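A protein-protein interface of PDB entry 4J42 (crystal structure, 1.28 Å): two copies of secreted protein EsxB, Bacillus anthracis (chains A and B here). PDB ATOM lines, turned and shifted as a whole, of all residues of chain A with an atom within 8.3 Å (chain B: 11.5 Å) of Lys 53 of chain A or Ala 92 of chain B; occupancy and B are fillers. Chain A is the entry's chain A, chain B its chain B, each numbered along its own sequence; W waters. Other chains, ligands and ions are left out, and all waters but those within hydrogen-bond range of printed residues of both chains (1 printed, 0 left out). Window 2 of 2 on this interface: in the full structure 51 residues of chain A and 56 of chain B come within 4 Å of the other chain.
The side-chain carboxylate of Glu 57 of chain A lies within hydrogen-bond range of the side-chain hydroxyl of Thr 89 of chain B, at 2.6 Å. O of Lys 85 of chain B sits close to OE2 of Glu 57 of chain A, 3.5 Å away. The side-chain amino group (NZ) of Lys 53 of chain A sits close to the backbone carbonyl oxygen (O) of Thr 89 of chain B (3.5 Å).
O of Lys 85 of chain B sits at hydrogen-bond distance from OG1 of Thr 89 of chain B (3.0 Å). NE2 of Gln 51 of chain A lies close to O of Trp 46 of chain A.
O of Ile 9 of chain B touches NE1 of Trp 46 of chain A, 3.5 Å away. Pro 11 of chain B touches Trp 46 of chain A (CD to CG, 3.4 Å). NZ of Lys 53 of chain A touches O of Ala 92 of chain B, at 3.8 Å. CE1 of Phe 86 of chain B touches CD1 of Phe 54 of chain A, 3.6 Å away. CE1 of Phe 54 of chain A touches CG2 of Thr 89 of chain B, 3.7 Å away. Asp 90 of chain B touches Phe 54 of chain A. CE2 of Phe 86 of chain B touches CB of Glu 57 of chain A (3.6 Å). Phe 58 of chain A touches Ile 9 of chain B (CD2 to O, 3.8 Å). Phe 58 of chain A touches Pro 11 of chain B (CE2 to N, 3.5 Å). Phe 58 of chain A touches Leu 14 of chain B (CG to CD1, 3.4 Å).
Of the printed residues of chain B, Lys 53 of chain A touches Thr 89, Asp 90 and Ala 92. Ala 49 of chain A touches none of the printed residues of chain B. Printed residues of chain A within 4 Å of Phe 86 of chain B: Phe 54 (3.6 Å), Glu 57 (3.6 Å) and Phe 58 (3.7 Å). Of the printed residues of chain B, Trp 46 of chain A touches Ile 9 (3.5 Å) and Pro 11 (3.4 Å). Of the printed residues of chain B, Glu 57 of chain A touches Lys 85, Phe 86 and Thr 89. Printed residues of chain A within 4 Å of Lys 85 of chain B: Glu 57 (3.5 Å). Asp 84 of chain B touches none of the printed residues of chain A. The nearest printed residue of chain A that does not touch Phe 86 of chain B is Leu 42 of chain A (4.1 Å).
Of the 14 printed residues of chain A, 5 touch a printed residue of chain B.
No position is printed for both chains.
Water W1 lies within hydrogen-bond range of NE1 of Trp 46 of chain A (2.8 Å) and O of Ile 9 of chain B (3.0 Å).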
ATOM      1  N   LEU A  42       9.183  -6.872   5.153  1.00  0.00           N
ATOM      2  CA  LEU A  42      10.430  -6.726   5.889  1.00  0.00           C
ATOM      3  C   LEU A  42      11.481  -7.794   5.565  1.00  0.00           C
ATOM      4  O   LEU A  42      12.596  -7.721   6.078  1.00  0.00           O
ATOM      5  CB  LEU A  42      10.158  -6.711   7.394  1.00  0.00           C
ATOM      6  CG  LEU A  42       9.283  -5.561   7.886  1.00  0.00           C
ATOM      7  CD1 LEU A  42       9.052  -5.726   9.374  1.00  0.00           C
ATOM      8  CD2 LEU A  42       9.924  -4.216   7.592  1.00  0.00           C
ATOM      9  N   TRP A  46      15.567  -7.001   7.362  1.00  0.00           N
ATOM     10  CA  TRP A  46      15.612  -7.281   8.790  1.00  0.00           C
ATOM     11  C   TRP A  46      17.026  -7.137   9.337  1.00  0.00           C
ATOM     12  O   TRP A  46      17.732  -8.123   9.554  1.00  0.00           O
ATOM     13  CB  TRP A  46      15.030  -8.664   9.101  1.00  0.00           C
ATOM     14  CG  TRP A  46      14.646  -8.838  10.534  1.00  0.00           C
ATOM     15  CD1 TRP A  46      15.217  -9.684  11.448  1.00  0.00           C
ATOM     16  CD2 TRP A  46      13.599  -8.149  11.234  1.00  0.00           C
ATOM     17  NE1 TRP A  46      14.588  -9.560  12.664  1.00  0.00           N
ATOM     18  CE2 TRP A  46      13.590  -8.627  12.554  1.00  0.00           C
ATOM     19  CE3 TRP A  46      12.667  -7.176  10.853  1.00  0.00           C
ATOM     20  CZ2 TRP A  46      12.690  -8.151  13.512  1.00  0.00           C
ATOM     21  CZ3 TRP A  46      11.769  -6.716  11.801  1.00  0.00           C
ATOM     22  CH2 TRP A  46      11.786  -7.202  13.115  1.00  0.00           C
ATOM     23  N   ALA A  47      17.422  -5.889   9.553  1.00  0.00           N
ATOM     24  CA  ALA A  47      18.758  -5.563  10.024  1.00  0.00           C
ATOM     25  C   ALA A  47      18.717  -4.149  10.565  1.00  0.00           C
ATOM     26  O   ALA A  47      17.793  -3.391  10.272  1.00  0.00           O
ATOM     27  CB  ALA A  47      19.757  -5.667   8.885  1.00  0.00           C
ATOM     28  N   GLY A  48      19.713  -3.802  11.371  1.00  0.00           N
ATOM     29  CA  GLY A  48      19.848  -2.446  11.863  1.00  0.00           C
ATOM     30  C   GLY A  48      18.611  -1.912  12.558  1.00  0.00           C
ATOM     31  O   GLY A  48      17.931  -2.628  13.295  1.00  0.00           O
ATOM     32  N   ALA A  49      18.318  -0.643  12.294  1.00  0.00           N
ATOM     33  CA  ALA A  49      17.245   0.068  12.970  1.00  0.00           C
ATOM     34  C   ALA A  49      15.884  -0.564  12.709  1.00  0.00           C
ATOM     35  O   ALA A  49      14.989  -0.474  13.547  1.00  0.00           O
ATOM     36  CB  ALA A  49      17.245   1.534  12.551  1.00  0.00           C
ATOM     37  N   THR A  50      15.730  -1.206  11.551  1.00  0.00           N
ATOM     38  CA  THR A  50      14.459  -1.837  11.194  1.00  0.00           C
ATOM     39  C   THR A  50      14.117  -2.968  12.160  1.00  0.00           C
ATOM     40  O   THR A  50      12.972  -3.089  12.598  1.00  0.00           O
ATOM     41  CB  THR A  50      14.481  -2.360   9.742  1.00  0.00           C
ATOM     42  OG1 THR A  50      14.678  -1.258   8.849  1.00  0.00           O
ATOM     43  CG2 THR A  50      13.172  -3.056   9.394  1.00  0.00           C
ATOM     44  N   GLN A  51      15.109  -3.797  12.484  1.00  0.00           N
ATOM     45  CA  GLN A  51      14.950  -4.856  13.482  1.00  0.00           C
ATOM     46  C   GLN A  51      14.433  -4.314  14.806  1.00  0.00           C
ATOM     47  O   GLN A  51      13.493  -4.846  15.384  1.00  0.00           O
ATOM     48  CB  GLN A  51      16.289  -5.527  13.772  1.00  0.00           C
ATOM     49  CG  GLN A  51      16.684  -6.659  12.855  1.00  0.00           C
ATOM     50  CD  GLN A  51      17.897  -7.401  13.388  1.00  0.00           C
ATOM     51  OE1 GLN A  51      18.653  -6.868  14.203  1.00  0.00           O
ATOM     52  NE2 GLN A  51      18.086  -8.634  12.934  1.00  0.00           N
ATOM     53  N   ALA A  52      15.081  -3.268  15.306  1.00  0.00           N
ATOM     54  CA  ALA A  52      14.718  -2.720  16.605  1.00  0.00           C
ATOM     55  C   ALA A  52      13.322  -2.117  16.557  1.00  0.00           C
ATOM     56  O   ALA A  52      12.530  -2.268  17.488  1.00  0.00           O
ATOM     57  CB  ALA A  52      15.734  -1.676  17.040  1.00  0.00           C
ATOM     58  N   LYS A  53      13.028  -1.446  15.449  1.00  0.00           N
ATOM     59  CA  LYS A  53      11.765  -0.748  15.265  1.00  0.00           C
ATOM     60  C   LYS A  53      10.569  -1.684  15.325  1.00  0.00           C
ATOM     61  O   LYS A  53       9.542  -1.352  15.916  1.00  0.00           O
ATOM     62  CB  LYS A  53      11.771  -0.015  13.922  1.00  0.00           C
ATOM     63  CG  LYS A  53      10.583   0.910  13.705  1.00  0.00           C
ATOM     64  CD  LYS A  53      10.712   1.673  12.389  1.00  0.00           C
ATOM     65  CE  LYS A  53       9.915   2.968  12.413  1.00  0.00           C
ATOM     66  NZ  LYS A  53       9.983   3.704  11.115  1.00  0.00           N
ATOM     67  N   PHE A  54      10.697  -2.863  14.720  1.00  0.00           N
ATOM     68  CA  PHE A  54       9.559  -3.754  14.570  1.00  0.00           C
ATOM     69  C   PHE A  54       9.611  -4.989  15.461  1.00  0.00           C
ATOM     70  O   PHE A  54       8.740  -5.841  15.371  1.00  0.00           O
ATOM     71  CB  PHE A  54       9.391  -4.164  13.103  1.00  0.00           C
ATOM     72  CG  PHE A  54       8.951  -3.041  12.213  1.00  0.00           C
ATOM     73  CD1 PHE A  54       7.625  -2.629  12.194  1.00  0.00           C
ATOM     74  CD2 PHE A  54       9.860  -2.398  11.395  1.00  0.00           C
ATOM     75  CE1 PHE A  54       7.219  -1.582  11.374  1.00  0.00           C
ATOM     76  CE2 PHE A  54       9.464  -1.350  10.571  1.00  0.00           C
ATOM     77  CZ  PHE A  54       8.137  -0.947  10.559  1.00  0.00           C
ATOM     78  N   ARG A  55      10.615  -5.071  16.330  1.00  0.00           N
ATOM     79  CA  ARG A  55      10.761  -6.222  17.224  1.00  0.00           C
ATOM     80  C   ARG A  55       9.491  -6.519  18.020  1.00  0.00           C
ATOM     81  O   ARG A  55       9.064  -7.669  18.122  1.00  0.00           O
ATOM     82  CB  ARG A  55      11.922  -6.028  18.204  1.00  0.00           C
ATOM     83  CG  ARG A  55      12.189  -7.281  19.028  1.00  0.00           C
ATOM     84  CD  ARG A  55      12.722  -6.990  20.419  1.00  0.00           C
ATOM     85  NE  ARG A  55      12.835  -8.228  21.187  1.00  0.00           N
ATOM     86  CZ  ARG A  55      13.123  -8.292  22.483  1.00  0.00           C
ATOM     87  NH1 ARG A  55      13.330  -7.181  23.177  1.00  0.00           N
ATOM     88  NH2 ARG A  55      13.199  -9.469  23.088  1.00  0.00           N
ATOM     89  N   GLY A  56       8.890  -5.474  18.582  1.00  0.00           N
ATOM     90  CA  GLY A  56       7.696  -5.632  19.392  1.00  0.00           C
ATOM     91  C   GLY A  56       6.551  -6.228  18.598  1.00  0.00           C
ATOM     92  O   GLY A  56       5.858  -7.137  19.065  1.00  0.00           O
ATOM     93  N   GLU A  57       6.345  -5.728  17.385  1.00  0.00           N
ATOM     94  CA  GLU A  57       5.290  -6.250  16.531  1.00  0.00           C
ATOM     95  C   GLU A  57       5.528  -7.707  16.161  1.00  0.00           C
ATOM     96  O   GLU A  57       4.584  -8.469  16.001  1.00  0.00           O
ATOM     97  CB  GLU A  57       5.146  -5.414  15.257  1.00  0.00           C
ATOM     98  CG  GLU A  57       4.404  -4.102  15.441  1.00  0.00           C
ATOM     99  CD  GLU A  57       5.309  -2.961  15.847  1.00  0.00           C
ATOM    100  OE1 GLU A  57       6.532  -3.178  16.004  1.00  0.00           O
ATOM    101  OE2 GLU A  57       4.794  -1.838  16.027  1.00  0.00           O
ATOM    102  N   PHE A  58       6.791  -8.093  16.013  1.00  0.00           N
ATOM    103  CA  PHE A  58       7.108  -9.486  15.720  1.00  0.00           C
ATOM    104  C   PHE A  58       6.776 -10.393  16.906  1.00  0.00           C
ATOM    105  O   PHE A  58       6.227 -11.480  16.725  1.00  0.00           O
ATOM    106  CB  PHE A  58       8.578  -9.639  15.302  1.00  0.00           C
ATOM    107  CG  PHE A  58       8.827  -9.412  13.830  1.00  0.00           C
ATOM    108  CD1 PHE A  58       7.976  -8.612  13.078  1.00  0.00           C
ATOM    109  CD2 PHE A  58       9.885 -10.040  13.193  1.00  0.00           C
ATOM    110  CE1 PHE A  58       8.197  -8.416  11.718  1.00  0.00           C
ATOM    111  CE2 PHE A  58      10.107  -9.853  11.830  1.00  0.00           C
ATOM    112  CZ  PHE A  58       9.257  -9.043  11.099  1.00  0.00           C
ATOM    113  N   ILE B   9      13.175 -13.527  16.907  1.00  0.00           N
ATOM    114  CA  ILE B   9      12.148 -13.806  15.913  1.00  0.00           C
ATOM    115  C   ILE B   9      12.512 -13.121  14.593  1.00  0.00           C
ATOM    116  O   ILE B   9      12.829 -11.929  14.569  1.00  0.00           O
ATOM    117  CB  ILE B   9      10.777 -13.303  16.395  1.00  0.00           C
ATOM    118  CG1 ILE B   9      10.410 -13.961  17.730  1.00  0.00           C
ATOM    119  CG2 ILE B   9       9.705 -13.581  15.361  1.00  0.00           C
ATOM    120  CD1 ILE B   9       9.218 -13.333  18.417  1.00  0.00           C
ATOM    121  N   PRO B  11      11.667 -12.542  10.180  1.00  0.00           N
ATOM    122  CA  PRO B  11      10.543 -12.587   9.240  1.00  0.00           C
ATOM    123  C   PRO B  11      10.308 -13.997   8.693  1.00  0.00           C
ATOM    124  O   PRO B  11       9.174 -14.355   8.426  1.00  0.00           O
ATOM    125  CB  PRO B  11      10.990 -11.651   8.110  1.00  0.00           C
ATOM    126  CG  PRO B  11      11.964 -10.719   8.749  1.00  0.00           C
ATOM    127  CD  PRO B  11      12.682 -11.541   9.786  1.00  0.00           C
ATOM    128  N   LEU B  14       8.248 -16.068  11.190  1.00  0.00           N
ATOM    129  CA  LEU B  14       6.891 -15.557  11.164  1.00  0.00           C
ATOM    130  C   LEU B  14       6.156 -15.929   9.888  1.00  0.00           C
ATOM    131  O   LEU B  14       4.966 -16.160   9.930  1.00  0.00           O
ATOM    132  CB  LEU B  14       6.855 -14.041  11.360  1.00  0.00           C
ATOM    133  CG  LEU B  14       7.173 -13.537  12.762  1.00  0.00           C
ATOM    134  CD1 LEU B  14       6.949 -12.042  12.824  1.00  0.00           C
ATOM    135  CD2 LEU B  14       6.329 -14.253  13.817  1.00  0.00           C
ATOM    136  N   ILE B  82      -2.688  -5.501  15.735  1.00  0.00           N
ATOM    137  CA  ILE B  82      -1.260  -5.669  15.483  1.00  0.00           C
ATOM    138  C   ILE B  82      -0.878  -5.046  14.141  1.00  0.00           C
ATOM    139  O   ILE B  82       0.104  -4.312  14.043  1.00  0.00           O
ATOM    140  CB  ILE B  82      -0.834  -7.153  15.511  1.00  0.00           C
ATOM    141  CG1 ILE B  82      -1.162  -7.779  16.864  1.00  0.00           C
ATOM    142  CG2 ILE B  82       0.647  -7.284  15.204  1.00  0.00           C
ATOM    143  CD1 ILE B  82      -0.936  -9.280  16.906  1.00  0.00           C
ATOM    144  N   ALA B  83      -1.671  -5.332  13.110  1.00  0.00           N
ATOM    145  CA  ALA B  83      -1.428  -4.735  11.797  1.00  0.00           C
ATOM    146  C   ALA B  83      -1.504  -3.203  11.834  1.00  0.00           C
ATOM    147  O   ALA B  83      -0.739  -2.527  11.152  1.00  0.00           O
ATOM    148  CB  ALA B  83      -2.398  -5.297  10.778  1.00  0.00           C
ATOM    149  N   ASP B  84      -2.429  -2.662  12.626  1.00  0.00           N
ATOM    150  CA  ASP B  84      -2.536  -1.211  12.781  1.00  0.00           C
ATOM    151  C   ASP B  84      -1.292  -0.626  13.448  1.00  0.00           C
ATOM    152  O   ASP B  84      -0.804   0.421  13.033  1.00  0.00           O
ATOM    153  CB  ASP B  84      -3.781  -0.836  13.590  1.00  0.00           C
ATOM    154  CG  ASP B  84      -5.072  -1.048  12.823  1.00  0.00           C
ATOM    155  OD1 ASP B  84      -5.022  -1.302  11.602  1.00  0.00           O
ATOM    156  OD2 ASP B  84      -6.151  -0.954  13.447  1.00  0.00           O
ATOM    157  N   LYS B  85      -0.793  -1.300  14.486  1.00  0.00           N
ATOM    158  CA  LYS B  85       0.427  -0.871  15.169  1.00  0.00           C
ATOM    159  C   LYS B  85       1.590  -0.881  14.198  1.00  0.00           C
ATOM    160  O   LYS B  85       2.452  -0.010  14.241  1.00  0.00           O
ATOM    161  CB  LYS B  85       0.765  -1.789  16.344  1.00  0.00           C
ATOM    162  CG  LYS B  85      -0.155  -1.685  17.543  1.00  0.00           C
ATOM    163  CD  LYS B  85       0.457  -2.414  18.735  1.00  0.00           C
ATOM    164  CE  LYS B  85      -0.608  -2.883  19.711  1.00  0.00           C
ATOM    165  NZ  LYS B  85      -1.480  -3.926  19.108  1.00  0.00           N
ATOM    166  N   PHE B  86       1.613  -1.889  13.334  1.00  0.00           N
ATOM    167  CA  PHE B  86       2.623  -1.994  12.287  1.00  0.00           C
ATOM    168  C   PHE B  86       2.630  -0.723  11.452  1.00  0.00           C
ATOM    169  O   PHE B  86       3.671  -0.101  11.241  1.00  0.00           O
ATOM    170  CB  PHE B  86       2.305  -3.180  11.379  1.00  0.00           C
ATOM    171  CG  PHE B  86       3.243  -4.340  11.529  1.00  0.00           C
ATOM    172  CD1 PHE B  86       4.558  -4.243  11.099  1.00  0.00           C
ATOM    173  CD2 PHE B  86       2.804  -5.540  12.065  1.00  0.00           C
ATOM    174  CE1 PHE B  86       5.425  -5.315  11.230  1.00  0.00           C
ATOM    175  CE2 PHE B  86       3.667  -6.615  12.195  1.00  0.00           C
ATOM    176  CZ  PHE B  86       4.976  -6.502  11.775  1.00  0.00           C
ATOM    177  N   ARG B  87       1.447  -0.351  10.977  1.00  0.00           N
ATOM    178  CA  ARG B  87       1.255   0.844  10.166  1.00  0.00           C
ATOM    179  C   ARG B  87       1.695   2.100  10.913  1.00  0.00           C
ATOM    180  O   ARG B  87       2.441   2.915  10.375  1.00  0.00           O
ATOM    181  CB  ARG B  87      -0.218   0.952   9.773  1.00  0.00           C
ATOM    182  CG  ARG B  87      -0.560   2.103   8.846  1.00  0.00           C
ATOM    183  CD  ARG B  87      -2.066   2.187   8.675  1.00  0.00           C
ATOM    184  NE  ARG B  87      -2.736   2.356   9.962  1.00  0.00           N
ATOM    185  CZ  ARG B  87      -4.027   2.121  10.174  1.00  0.00           C
ATOM    186  NH1 ARG B  87      -4.798   1.694   9.183  1.00  0.00           N
ATOM    187  NH2 ARG B  87      -4.549   2.303  11.380  1.00  0.00           N
ATOM    188  N   ASN B  88       1.242   2.241  12.156  1.00  0.00           N
ATOM    189  CA  ASN B  88       1.592   3.399  12.976  1.00  0.00           C
ATOM    190  C   ASN B  88       3.090   3.505  13.248  1.00  0.00           C
ATOM    191  O   ASN B  88       3.659   4.593  13.207  1.00  0.00           O
ATOM    192  CB  ASN B  88       0.835   3.364  14.303  1.00  0.00           C
ATOM    193  CG  ASN B  88      -0.665   3.477  14.124  1.00  0.00           C
ATOM    194  OD1 ASN B  88      -1.147   3.911  13.076  1.00  0.00           O
ATOM    195  ND2 ASN B  88      -1.412   3.093  15.151  1.00  0.00           N
ATOM    196  N   THR B  89       3.717   2.372  13.543  1.00  0.00           N
ATOM    197  CA  THR B  89       5.151   2.328  13.802  1.00  0.00           C
ATOM    198  C   THR B  89       5.917   2.715  12.549  1.00  0.00           C
ATOM    199  O   THR B  89       6.851   3.513  12.597  1.00  0.00           O
ATOM    200  CB  THR B  89       5.584   0.919  14.238  1.00  0.00           C
ATOM    201  OG1 THR B  89       5.088   0.657  15.556  1.00  0.00           O
ATOM    202  CG2 THR B  89       7.095   0.796  14.237  1.00  0.00           C
ATOM    203  N   ASP B  90       5.493   2.156  11.423  1.00  0.00           N
ATOM    204  CA  ASP B  90       6.148   2.392  10.148  1.00  0.00           C
ATOM    205  C   ASP B  90       6.009   3.846   9.695  1.00  0.00           C
ATOM    206  O   ASP B  90       6.890   4.376   9.014  1.00  0.00           O
ATOM    207  CB  ASP B  90       5.559   1.456   9.099  1.00  0.00           C
ATOM    208  CG  ASP B  90       6.326   1.477   7.806  1.00  0.00           C
ATOM    209  OD1 ASP B  90       7.569   1.359   7.833  1.00  0.00           O
ATOM    210  OD2 ASP B  90       5.674   1.618   6.758  1.00  0.00           O
ATOM    211  N   ASN B  91       4.908   4.487  10.080  1.00  0.00           N
ATOM    212  CA  ASN B  91       4.638   5.868   9.680  1.00  0.00           C
ATOM    213  C   ASN B  91       5.300   6.912  10.578  1.00  0.00           C
ATOM    214  O   ASN B  91       5.451   8.069  10.185  1.00  0.00           O
ATOM    215  CB  ASN B  91       3.129   6.131   9.607  1.00  0.00           C
ATOM    216  CG  ASN B  91       2.467   5.437   8.429  1.00  0.00           C
ATOM    217  OD1 ASN B  91       3.141   4.946   7.521  1.00  0.00           O
ATOM    218  ND2 ASN B  91       1.139   5.408   8.430  1.00  0.00           N
ATOM    219  N   ALA B  92       5.688   6.503  11.782  1.00  0.00           N
ATOM    220  CA  ALA B  92       6.317   7.412  12.736  1.00  0.00           C
ATOM    221  C   ALA B  92       7.663   7.925  12.229  1.00  0.00           C
ATOM    222  O   ALA B  92       8.564   7.142  11.922  1.00  0.00           O
ATOM    223  CB  ALA B  92       6.484   6.731  14.084  1.00  0.00           C
HETATM  224  O   HOH W   1      15.792 -11.292  14.478  1.00  0.00           O
